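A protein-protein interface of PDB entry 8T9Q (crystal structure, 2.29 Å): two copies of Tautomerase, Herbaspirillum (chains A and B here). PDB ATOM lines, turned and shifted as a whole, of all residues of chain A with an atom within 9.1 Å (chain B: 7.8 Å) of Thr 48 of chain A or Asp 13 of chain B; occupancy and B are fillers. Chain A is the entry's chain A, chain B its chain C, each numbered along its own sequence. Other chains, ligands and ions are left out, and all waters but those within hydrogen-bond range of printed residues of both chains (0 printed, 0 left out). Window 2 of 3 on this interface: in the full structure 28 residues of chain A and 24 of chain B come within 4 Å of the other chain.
The backbone carbonyl oxygen of Val 40 of chain B sits at hydrogen-bond distance from the backbone NH of Gly 51 of chain A (2.7 Å).
The backbone carbonyl oxygen (O) of Gln 49 of chain A lies within hydrogen-bond range of the backbone NH (N) of Leu 42 of chain B, at 3.0 Å.
OE1 of Gln 49 of chain A sits close to OE2 of Glu 44 of chain B (3.2 Å).
OG1 of Thr 56 of chain A sits close to N of Ala 58 of chain A.
The side-chain amino group of Lys 16 of chain B is in hydrogen-bond range of the backbone carbonyl oxygen of Tyr 11 of chain B.
The side-chain carboxylate (OD1) of Asp 13 of chain B is in salt-bridge range of the side-chain amino group (NZ) of Lys 16 of chain B, at 3.2 Å.
NE2 of Gln 14 of chain B sits at hydrogen-bond distance from OE2 of Glu 17 of chain B, at 3.1 Å.
NZ of Lys 16 of chain B lies within salt-bridge range of OE2 of Glu 44 of chain B, 3.5 Å away.
OG1 of Thr 56 of chain A sits at hydrogen-bond distance from N of Ala 59 of chain A (3.0 Å).
Thr 48 of chain A touches Asp 13 of chain B (CG2 to OD2, 3.8 Å).
CB of Lys 16 of chain B touches O of Thr 48 of chain A, 3.6 Å away.
CD of Lys 16 of chain B touches CG of Gln 49 of chain A, at 3.9 Å.
Gln 49 of chain A touches Val 40 of chain B.
O of Val 40 of chain B touches C of Phe 50 of chain A, at 3.6 Å.
Gly 51 of chain A touches Val 20 of chain B (CA to CG1, 3.6 Å).
Thr 56 of chain A touches Glu 17 of chain B (CG2 to CB, 3.5 Å).
Of the printed residues of chain B, Gln 49 of chain A touches Lys 16 (3.9 Å), Val 40 (3.9 Å), Leu 42 (3.0 Å) and Glu 44 (3.2 Å).
Lys 55 of chain A touches none of the printed residues of chain B.
No residue of chain A comes within 4 Å of Ser 12 of chain B.
Of the printed residues of chain A, Asp 13 of chain B touches Thr 48 (3.8 Å).
Of chain A, only Thr 48 (3.6 Å) and Gln 49 (3.9 Å) come within 4 Å of Lys 16 of chain B.
Leu 19 of chain B touches none of the printed residues of chain A.
Printed residues of chain A within 4 Å of Val 40 of chain B: Gln 49 (3.9 Å), Phe 50 (3.6 Å) and Gly 51 (2.7 Å).
The nearest residue of chain B that does not touch Thr 48 of chain A is Leu 42 of chain B (4.6 Å).
The nearest residue of chain A that does not touch Asp 13 of chain B is Thr 56 of chain A (5.8 Å).
The nearest printed residue of chain A that does not touch Val 40 of chain B is Val 45 of chain A (6.2 Å).
Of the 14 printed residues of chain B, 7 touch a printed residue of chain A.
Hydrophobic or aromatic side chains of chain B that line the printed part of chain A: Val 20 and Leu 42.
Printed residues of chain A that touch a printed residue of chain B: Thr 48, Gln 49, Phe 50, Gly 51 and Thr 56.
Hydrophobic or aromatic side chains of chain A that line the printed part of chain B: Phe 50.
Among the printed residues, no Asp or Glu carboxylate lies within 4 Å of a Lys or Arg side-chain nitrogen of the other chain.
No position is printed for both chains.
Of the 10 pairs that touch across the chains among the printed residues, none has its exchanged pair printed and touching as well.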
ATOM      1  N   VAL A   8      -5.905   1.395  21.825  1.00  0.00           N
ATOM      2  CA  VAL A   8      -6.581   0.061  21.786  1.00  0.00           C
ATOM      3  C   VAL A   8      -7.785   0.166  20.841  1.00  0.00           C
ATOM      4  O   VAL A   8      -8.302   1.282  20.668  1.00  0.00           O
ATOM      5  CB  VAL A   8      -6.984  -0.450  23.186  1.00  0.00           C
ATOM      6  CG1 VAL A   8      -7.197  -1.964  23.202  1.00  0.00           C
ATOM      7  CG2 VAL A   8      -5.971  -0.056  24.250  1.00  0.00           C
ATOM      8  N   GLU A   9      -8.220  -0.966  20.277  1.00  0.00           N
ATOM      9  CA  GLU A   9      -9.150  -1.056  19.121  1.00  0.00           C
ATOM     10  C   GLU A   9     -10.623  -0.965  19.557  1.00  0.00           C
ATOM     11  O   GLU A   9     -11.444  -1.696  18.966  1.00  0.00           O
ATOM     12  CB  GLU A   9      -8.888  -2.374  18.386  1.00  0.00           C
ATOM     13  N   VAL A  45      -4.337  -1.065  18.185  1.00  0.00           N
ATOM     14  CA  VAL A  45      -3.682  -2.299  18.699  1.00  0.00           C
ATOM     15  C   VAL A  45      -4.766  -3.117  19.383  1.00  0.00           C
ATOM     16  O   VAL A  45      -5.444  -2.609  20.286  1.00  0.00           O
ATOM     17  CB  VAL A  45      -2.513  -1.994  19.644  1.00  0.00           C
ATOM     18  CG1 VAL A  45      -1.759  -3.268  19.992  1.00  0.00           C
ATOM     19  CG2 VAL A  45      -1.580  -0.938  19.072  1.00  0.00           C
ATOM     20  N   PRO A  46      -5.007  -4.373  18.936  1.00  0.00           N
ATOM     21  CA  PRO A  46      -5.956  -5.255  19.623  1.00  0.00           C
ATOM     22  C   PRO A  46      -5.428  -5.642  21.020  1.00  0.00           C
ATOM     23  O   PRO A  46      -4.236  -5.618  21.260  1.00  0.00           O
ATOM     24  CB  PRO A  46      -6.097  -6.471  18.677  1.00  0.00           C
ATOM     25  CG  PRO A  46      -5.423  -6.047  17.374  1.00  0.00           C
ATOM     26  CD  PRO A  46      -4.369  -5.040  17.779  1.00  0.00           C
ATOM     27  N   ALA A  47      -6.344  -5.966  21.927  1.00  0.00           N
ATOM     28  CA  ALA A  47      -6.109  -5.981  23.390  1.00  0.00           C
ATOM     29  C   ALA A  47      -5.059  -7.039  23.721  1.00  0.00           C
ATOM     30  O   ALA A  47      -4.137  -6.765  24.516  1.00  0.00           O
ATOM     31  CB  ALA A  47      -7.414  -6.226  24.096  1.00  0.00           C
ATOM     32  N   THR A  48      -5.186  -8.194  23.071  1.00  0.00           N
ATOM     33  CA  THR A  48      -4.221  -9.318  23.060  1.00  0.00           C
ATOM     34  C   THR A  48      -2.834  -8.822  22.649  1.00  0.00           C
ATOM     35  O   THR A  48      -1.877  -9.582  22.837  1.00  0.00           O
ATOM     36  CB  THR A  48      -4.727 -10.438  22.131  1.00  0.00           C
ATOM     37  OG1 THR A  48      -5.114  -9.836  20.898  1.00  0.00           O
ATOM     38  CG2 THR A  48      -5.930 -11.184  22.674  1.00  0.00           C
ATOM     39  N   GLN A  49      -2.686  -7.619  22.083  1.00  0.00           N
ATOM     40  CA  GLN A  49      -1.374  -7.212  21.530  1.00  0.00           C
ATOM     41  C   GLN A  49      -0.835  -5.962  22.236  1.00  0.00           C
ATOM     42  O   GLN A  49       0.220  -5.453  21.815  1.00  0.00           O
ATOM     43  CB  GLN A  49      -1.503  -7.035  20.016  1.00  0.00           C
ATOM     44  CG  GLN A  49      -1.769  -8.344  19.288  1.00  0.00           C
ATOM     45  CD  GLN A  49      -1.992  -8.147  17.810  1.00  0.00           C
ATOM     46  OE1 GLN A  49      -2.988  -8.597  17.250  1.00  0.00           O
ATOM     47  NE2 GLN A  49      -1.068  -7.448  17.175  1.00  0.00           N
ATOM     48  N   PHE A  50      -1.467  -5.503  23.307  1.00  0.00           N
ATOM     49  CA  PHE A  50      -1.016  -4.260  23.986  1.00  0.00           C
ATOM     50  C   PHE A  50      -0.771  -4.572  25.461  1.00  0.00           C
ATOM     51  O   PHE A  50      -1.720  -4.961  26.175  1.00  0.00           O
ATOM     52  CB  PHE A  50      -2.026  -3.137  23.728  1.00  0.00           C
ATOM     53  CG  PHE A  50      -1.496  -1.721  23.817  1.00  0.00           C
ATOM     54  CD1 PHE A  50      -0.195  -1.432  24.206  1.00  0.00           C
ATOM     55  CD2 PHE A  50      -2.332  -0.653  23.509  1.00  0.00           C
ATOM     56  CE1 PHE A  50       0.260  -0.120  24.246  1.00  0.00           C
ATOM     57  CE2 PHE A  50      -1.888   0.660  23.579  1.00  0.00           C
ATOM     58  CZ  PHE A  50      -0.582   0.925  23.926  1.00  0.00           C
ATOM     59  N   GLY A  51       0.484  -4.479  25.899  1.00  0.00           N
ATOM     60  CA  GLY A  51       0.887  -4.955  27.243  1.00  0.00           C
ATOM     61  C   GLY A  51       1.335  -3.827  28.160  1.00  0.00           C
ATOM     62  O   GLY A  51       2.148  -3.011  27.696  1.00  0.00           O
ATOM     63  N   LYS A  55       1.309  -7.654  31.337  1.00  0.00           N
ATOM     64  CA  LYS A  55       0.027  -8.364  31.072  1.00  0.00           C
ATOM     65  C   LYS A  55      -0.675  -7.691  29.892  1.00  0.00           C
ATOM     66  O   LYS A  55      -0.532  -6.478  29.750  1.00  0.00           O
ATOM     67  CB  LYS A  55      -0.870  -8.335  32.312  1.00  0.00           C
ATOM     68  CG  LYS A  55      -0.299  -9.031  33.541  1.00  0.00           C
ATOM     69  CD  LYS A  55      -1.345  -9.761  34.367  1.00  0.00           C
ATOM     70  CE  LYS A  55      -1.887 -11.005  33.693  1.00  0.00           C
ATOM     71  NZ  LYS A  55      -3.094 -11.512  34.388  1.00  0.00           N
ATOM     72  N   THR A  56      -1.435  -8.446  29.106  1.00  0.00           N
ATOM     73  CA  THR A  56      -2.106  -7.915  27.895  1.00  0.00           C
ATOM     74  C   THR A  56      -3.315  -7.176  28.414  1.00  0.00           C
ATOM     75  O   THR A  56      -3.877  -7.654  29.438  1.00  0.00           O
ATOM     76  CB  THR A  56      -2.515  -8.995  26.891  1.00  0.00           C
ATOM     77  OG1 THR A  56      -3.799  -9.515  27.228  1.00  0.00           O
ATOM     78  CG2 THR A  56      -1.535 -10.136  26.846  1.00  0.00           C
ATOM     79  N   VAL A  57      -3.707  -6.100  27.735  1.00  0.00           N
ATOM     80  CA  VAL A  57      -4.909  -5.322  28.143  1.00  0.00           C
ATOM     81  C   VAL A  57      -6.028  -6.327  28.392  1.00  0.00           C
ATOM     82  O   VAL A  57      -6.845  -6.099  29.338  1.00  0.00           O
ATOM     83  CB  VAL A  57      -5.313  -4.267  27.092  1.00  0.00           C
ATOM     84  CG1 VAL A  57      -6.549  -3.479  27.493  1.00  0.00           C
ATOM     85  CG2 VAL A  57      -4.179  -3.318  26.810  1.00  0.00           C
ATOM     86  N   ALA A  58      -6.127  -7.345  27.528  1.00  0.00           N
ATOM     87  CA  ALA A  58      -7.291  -8.252  27.491  1.00  0.00           C
ATOM     88  C   ALA A  58      -7.271  -9.055  28.783  1.00  0.00           C
ATOM     89  O   ALA A  58      -8.356  -9.227  29.343  1.00  0.00           O
ATOM     90  CB  ALA A  58      -7.258  -9.161  26.280  1.00  0.00           C
ATOM     91  N   ALA A  59      -6.076  -9.525  29.197  1.00  0.00           N
ATOM     92  CA  ALA A  59      -5.830 -10.275  30.451  1.00  0.00           C
ATOM     93  C   ALA A  59      -6.326  -9.422  31.614  1.00  0.00           C
ATOM     94  O   ALA A  59      -6.614  -9.970  32.690  1.00  0.00           O
ATOM     95  CB  ALA A  59      -4.362 -10.615  30.599  1.00  0.00           C
ATOM     96  N   ILE A  60      -6.486  -8.127  31.344  1.00  0.00           N
ATOM     97  CA  ILE A  60      -6.838  -7.074  32.327  1.00  0.00           C
ATOM     98  C   ILE A  60      -8.252  -6.582  32.011  1.00  0.00           C
ATOM     99  O   ILE A  60      -9.080  -7.443  31.619  1.00  0.00           O
ATOM    100  CB  ILE A  60      -5.744  -5.993  32.248  1.00  0.00           C
ATOM    101  CG1 ILE A  60      -4.506  -6.442  33.025  1.00  0.00           C
ATOM    102  CG2 ILE A  60      -6.239  -4.627  32.688  1.00  0.00           C
ATOM    103  CD1 ILE A  60      -3.279  -5.593  32.779  1.00  0.00           C
ATOM    104  N   GLY B  10       1.216 -14.834  11.891  1.00  0.00           N
ATOM    105  CA  GLY B  10       1.034 -16.222  12.374  1.00  0.00           C
ATOM    106  C   GLY B  10       0.671 -16.341  13.853  1.00  0.00           C
ATOM    107  O   GLY B  10      -0.203 -17.186  14.184  1.00  0.00           O
ATOM    108  N   TYR B  11       1.290 -15.535  14.723  1.00  0.00           N
ATOM    109  CA  TYR B  11       1.461 -15.816  16.182  1.00  0.00           C
ATOM    110  C   TYR B  11       0.093 -15.911  16.875  1.00  0.00           C
ATOM    111  O   TYR B  11      -0.849 -15.148  16.571  1.00  0.00           O
ATOM    112  CB  TYR B  11       2.454 -14.821  16.795  1.00  0.00           C
ATOM    113  CG  TYR B  11       3.844 -14.983  16.235  1.00  0.00           C
ATOM    114  CD1 TYR B  11       4.155 -14.548  14.958  1.00  0.00           C
ATOM    115  CD2 TYR B  11       4.844 -15.624  16.944  1.00  0.00           C
ATOM    116  CE1 TYR B  11       5.419 -14.711  14.415  1.00  0.00           C
ATOM    117  CE2 TYR B  11       6.118 -15.786  16.420  1.00  0.00           C
ATOM    118  CZ  TYR B  11       6.407 -15.334  15.145  1.00  0.00           C
ATOM    119  OH  TYR B  11       7.650 -15.476  14.597  1.00  0.00           O
ATOM    120  N   SER B  12      -0.042 -16.905  17.752  1.00  0.00           N
ATOM    121  CA  SER B  12      -1.280 -17.193  18.525  1.00  0.00           C
ATOM    122  C   SER B  12      -1.384 -16.232  19.710  1.00  0.00           C
ATOM    123  O   SER B  12      -0.366 -15.601  20.036  1.00  0.00           O
ATOM    124  CB  SER B  12      -1.270 -18.614  19.005  1.00  0.00           C
ATOM    125  OG  SER B  12      -0.181 -18.825  19.890  1.00  0.00           O
ATOM    126  N   ASP B  13      -2.554 -16.166  20.358  1.00  0.00           N
ATOM    127  CA  ASP B  13      -2.800 -15.317  21.563  1.00  0.00           C
ATOM    128  C   ASP B  13      -1.783 -15.657  22.672  1.00  0.00           C
ATOM    129  O   ASP B  13      -1.233 -14.706  23.302  1.00  0.00           O
ATOM    130  CB  ASP B  13      -4.248 -15.445  22.056  1.00  0.00           C
ATOM    131  CG  ASP B  13      -5.309 -14.711  21.236  1.00  0.00           C
ATOM    132  OD1 ASP B  13      -4.973 -14.085  20.201  1.00  0.00           O
ATOM    133  OD2 ASP B  13      -6.483 -14.767  21.648  1.00  0.00           O
ATOM    134  N   GLN B  14      -1.511 -16.946  22.903  1.00  0.00           N
ATOM    135  CA  GLN B  14      -0.567 -17.416  23.962  1.00  0.00           C
ATOM    136  C   GLN B  14       0.829 -16.841  23.700  1.00  0.00           C
ATOM    137  O   GLN B  14       1.444 -16.264  24.637  1.00  0.00           O
ATOM    138  CB  GLN B  14      -0.509 -18.942  23.996  1.00  0.00           C
ATOM    139  CG  GLN B  14       0.460 -19.501  25.033  1.00  0.00           C
ATOM    140  CD  GLN B  14       0.021 -19.154  26.434  1.00  0.00           C
ATOM    141  OE1 GLN B  14      -1.068 -19.531  26.863  1.00  0.00           O
ATOM    142  NE2 GLN B  14       0.854 -18.413  27.149  1.00  0.00           N
ATOM    143  N   GLN B  15       1.314 -17.013  22.470  1.00  0.00           N
ATOM    144  CA  GLN B  15       2.639 -16.508  22.018  1.00  0.00           C
ATOM    145  C   GLN B  15       2.703 -14.992  22.264  1.00  0.00           C
ATOM    146  O   GLN B  15       3.771 -14.499  22.677  1.00  0.00           O
ATOM    147  CB  GLN B  15       2.857 -16.863  20.543  1.00  0.00           C
ATOM    148  CG  GLN B  15       3.220 -18.327  20.316  1.00  0.00           C
ATOM    149  CD  GLN B  15       3.336 -18.686  18.852  1.00  0.00           C
ATOM    150  OE1 GLN B  15       2.487 -18.325  18.050  1.00  0.00           O
ATOM    151  NE2 GLN B  15       4.390 -19.398  18.485  1.00  0.00           N
ATOM    152  N   LYS B  16       1.599 -14.284  22.026  1.00  0.00           N
ATOM    153  CA  LYS B  16       1.524 -12.805  22.172  1.00  0.00           C
ATOM    154  C   LYS B  16       1.686 -12.459  23.653  1.00  0.00           C
ATOM    155  O   LYS B  16       2.542 -11.616  23.977  1.00  0.00           O
ATOM    156  CB  LYS B  16       0.196 -12.244  21.655  1.00  0.00           C
ATOM    157  CG  LYS B  16      -0.014 -12.321  20.147  1.00  0.00           C
ATOM    158  CD  LYS B  16      -1.469 -12.182  19.712  1.00  0.00           C
ATOM    159  CE  LYS B  16      -1.664 -12.479  18.235  1.00  0.00           C
ATOM    160  NZ  LYS B  16      -2.788 -13.414  17.978  1.00  0.00           N
ATOM    161  N   GLU B  17       0.902 -13.113  24.512  1.00  0.00           N
ATOM    162  CA  GLU B  17       0.852 -12.783  25.956  1.00  0.00           C
ATOM    163  C   GLU B  17       2.209 -13.171  26.558  1.00  0.00           C
ATOM    164  O   GLU B  17       2.758 -12.381  27.357  1.00  0.00           O
ATOM    165  CB  GLU B  17      -0.387 -13.408  26.606  1.00  0.00           C
ATOM    166  CG  GLU B  17      -0.189 -14.812  27.145  1.00  0.00           C
ATOM    167  CD  GLU B  17      -1.432 -15.395  27.794  1.00  0.00           C
ATOM    168  OE1 GLU B  17      -2.303 -14.609  28.223  1.00  0.00           O
ATOM    169  OE2 GLU B  17      -1.531 -16.632  27.860  1.00  0.00           O
ATOM    170  N   ALA B  18       2.794 -14.279  26.102  1.00  0.00           N
ATOM    171  CA  ALA B  18       4.140 -14.700  26.548  1.00  0.00           C
ATOM    172  C   ALA B  18       5.208 -13.737  25.996  1.00  0.00           C
ATOM    173  O   ALA B  18       6.151 -13.375  26.759  1.00  0.00           O
ATOM    174  CB  ALA B  18       4.372 -16.130  26.147  1.00  0.00           C
ATOM    175  N   LEU B  19       5.072 -13.301  24.736  1.00  0.00           N
ATOM    176  CA  LEU B  19       6.033 -12.346  24.124  1.00  0.00           C
ATOM    177  C   LEU B  19       5.995 -11.055  24.931  1.00  0.00           C
ATOM    178  O   LEU B  19       7.070 -10.495  25.207  1.00  0.00           O
ATOM    179  CB  LEU B  19       5.697 -12.090  22.649  1.00  0.00           C
ATOM    180  CG  LEU B  19       6.850 -11.634  21.752  1.00  0.00           C
ATOM    181  CD1 LEU B  19       8.163 -12.309  22.116  1.00  0.00           C
ATOM    182  CD2 LEU B  19       6.504 -11.909  20.294  1.00  0.00           C
ATOM    183  N   VAL B  20       4.801 -10.605  25.298  1.00  0.00           N
ATOM    184  CA  VAL B  20       4.627  -9.336  26.074  1.00  0.00           C
ATOM    185  C   VAL B  20       5.327  -9.479  27.440  1.00  0.00           C
ATOM    186  O   VAL B  20       6.186  -8.615  27.753  1.00  0.00           O
ATOM    187  CB  VAL B  20       3.136  -8.937  26.178  1.00  0.00           C
ATOM    188  CG1 VAL B  20       2.835  -8.012  27.344  1.00  0.00           C
ATOM    189  CG2 VAL B  20       2.650  -8.312  24.880  1.00  0.00           C
ATOM    190  N   VAL B  40       4.318  -2.361  26.028  1.00  0.00           N
ATOM    191  CA  VAL B  40       4.848  -3.212  24.927  1.00  0.00           C
ATOM    192  C   VAL B  40       3.704  -3.370  23.943  1.00  0.00           C
ATOM    193  O   VAL B  40       2.619  -3.759  24.415  1.00  0.00           O
ATOM    194  CB  VAL B  40       5.332  -4.579  25.431  1.00  0.00           C
ATOM    195  CG1 VAL B  40       5.882  -5.431  24.275  1.00  0.00           C
ATOM    196  CG2 VAL B  40       6.365  -4.433  26.539  1.00  0.00           C
ATOM    197  N   LEU B  42       2.681  -5.243  20.101  1.00  0.00           N
ATOM    198  CA  LEU B  42       3.032  -6.095  18.947  1.00  0.00           C
ATOM    199  C   LEU B  42       2.346  -5.544  17.679  1.00  0.00           C
ATOM    200  O   LEU B  42       1.118  -5.288  17.733  1.00  0.00           O
ATOM    201  CB  LEU B  42       2.551  -7.501  19.300  1.00  0.00           C
ATOM    202  CG  LEU B  42       2.994  -7.989  20.687  1.00  0.00           C
ATOM    203  CD1 LEU B  42       2.311  -9.310  21.045  1.00  0.00           C
ATOM    204  CD2 LEU B  42       4.499  -8.149  20.744  1.00  0.00           C
ATOM    205  N   GLU B  44       1.290  -6.847  14.061  1.00  0.00           N
ATOM    206  CA  GLU B  44       1.054  -7.945  13.089  1.00  0.00           C
ATOM    207  C   GLU B  44       1.029  -7.412  11.645  1.00  0.00           C
ATOM    208  O   GLU B  44       0.073  -6.671  11.319  1.00  0.00           O
ATOM    209  CB  GLU B  44      -0.310  -8.553  13.382  1.00  0.00           C
ATOM    210  CG  GLU B  44      -0.239  -9.625  14.435  1.00  0.00           C
ATOM    211  CD  GLU B  44      -1.546 -10.367  14.587  1.00  0.00           C
ATOM    212  OE1 GLU B  44      -2.425 -10.204  13.709  1.00  0.00           O
ATOM    213  OE2 GLU B  44      -1.693 -11.061  15.595  1.00  0.00           O
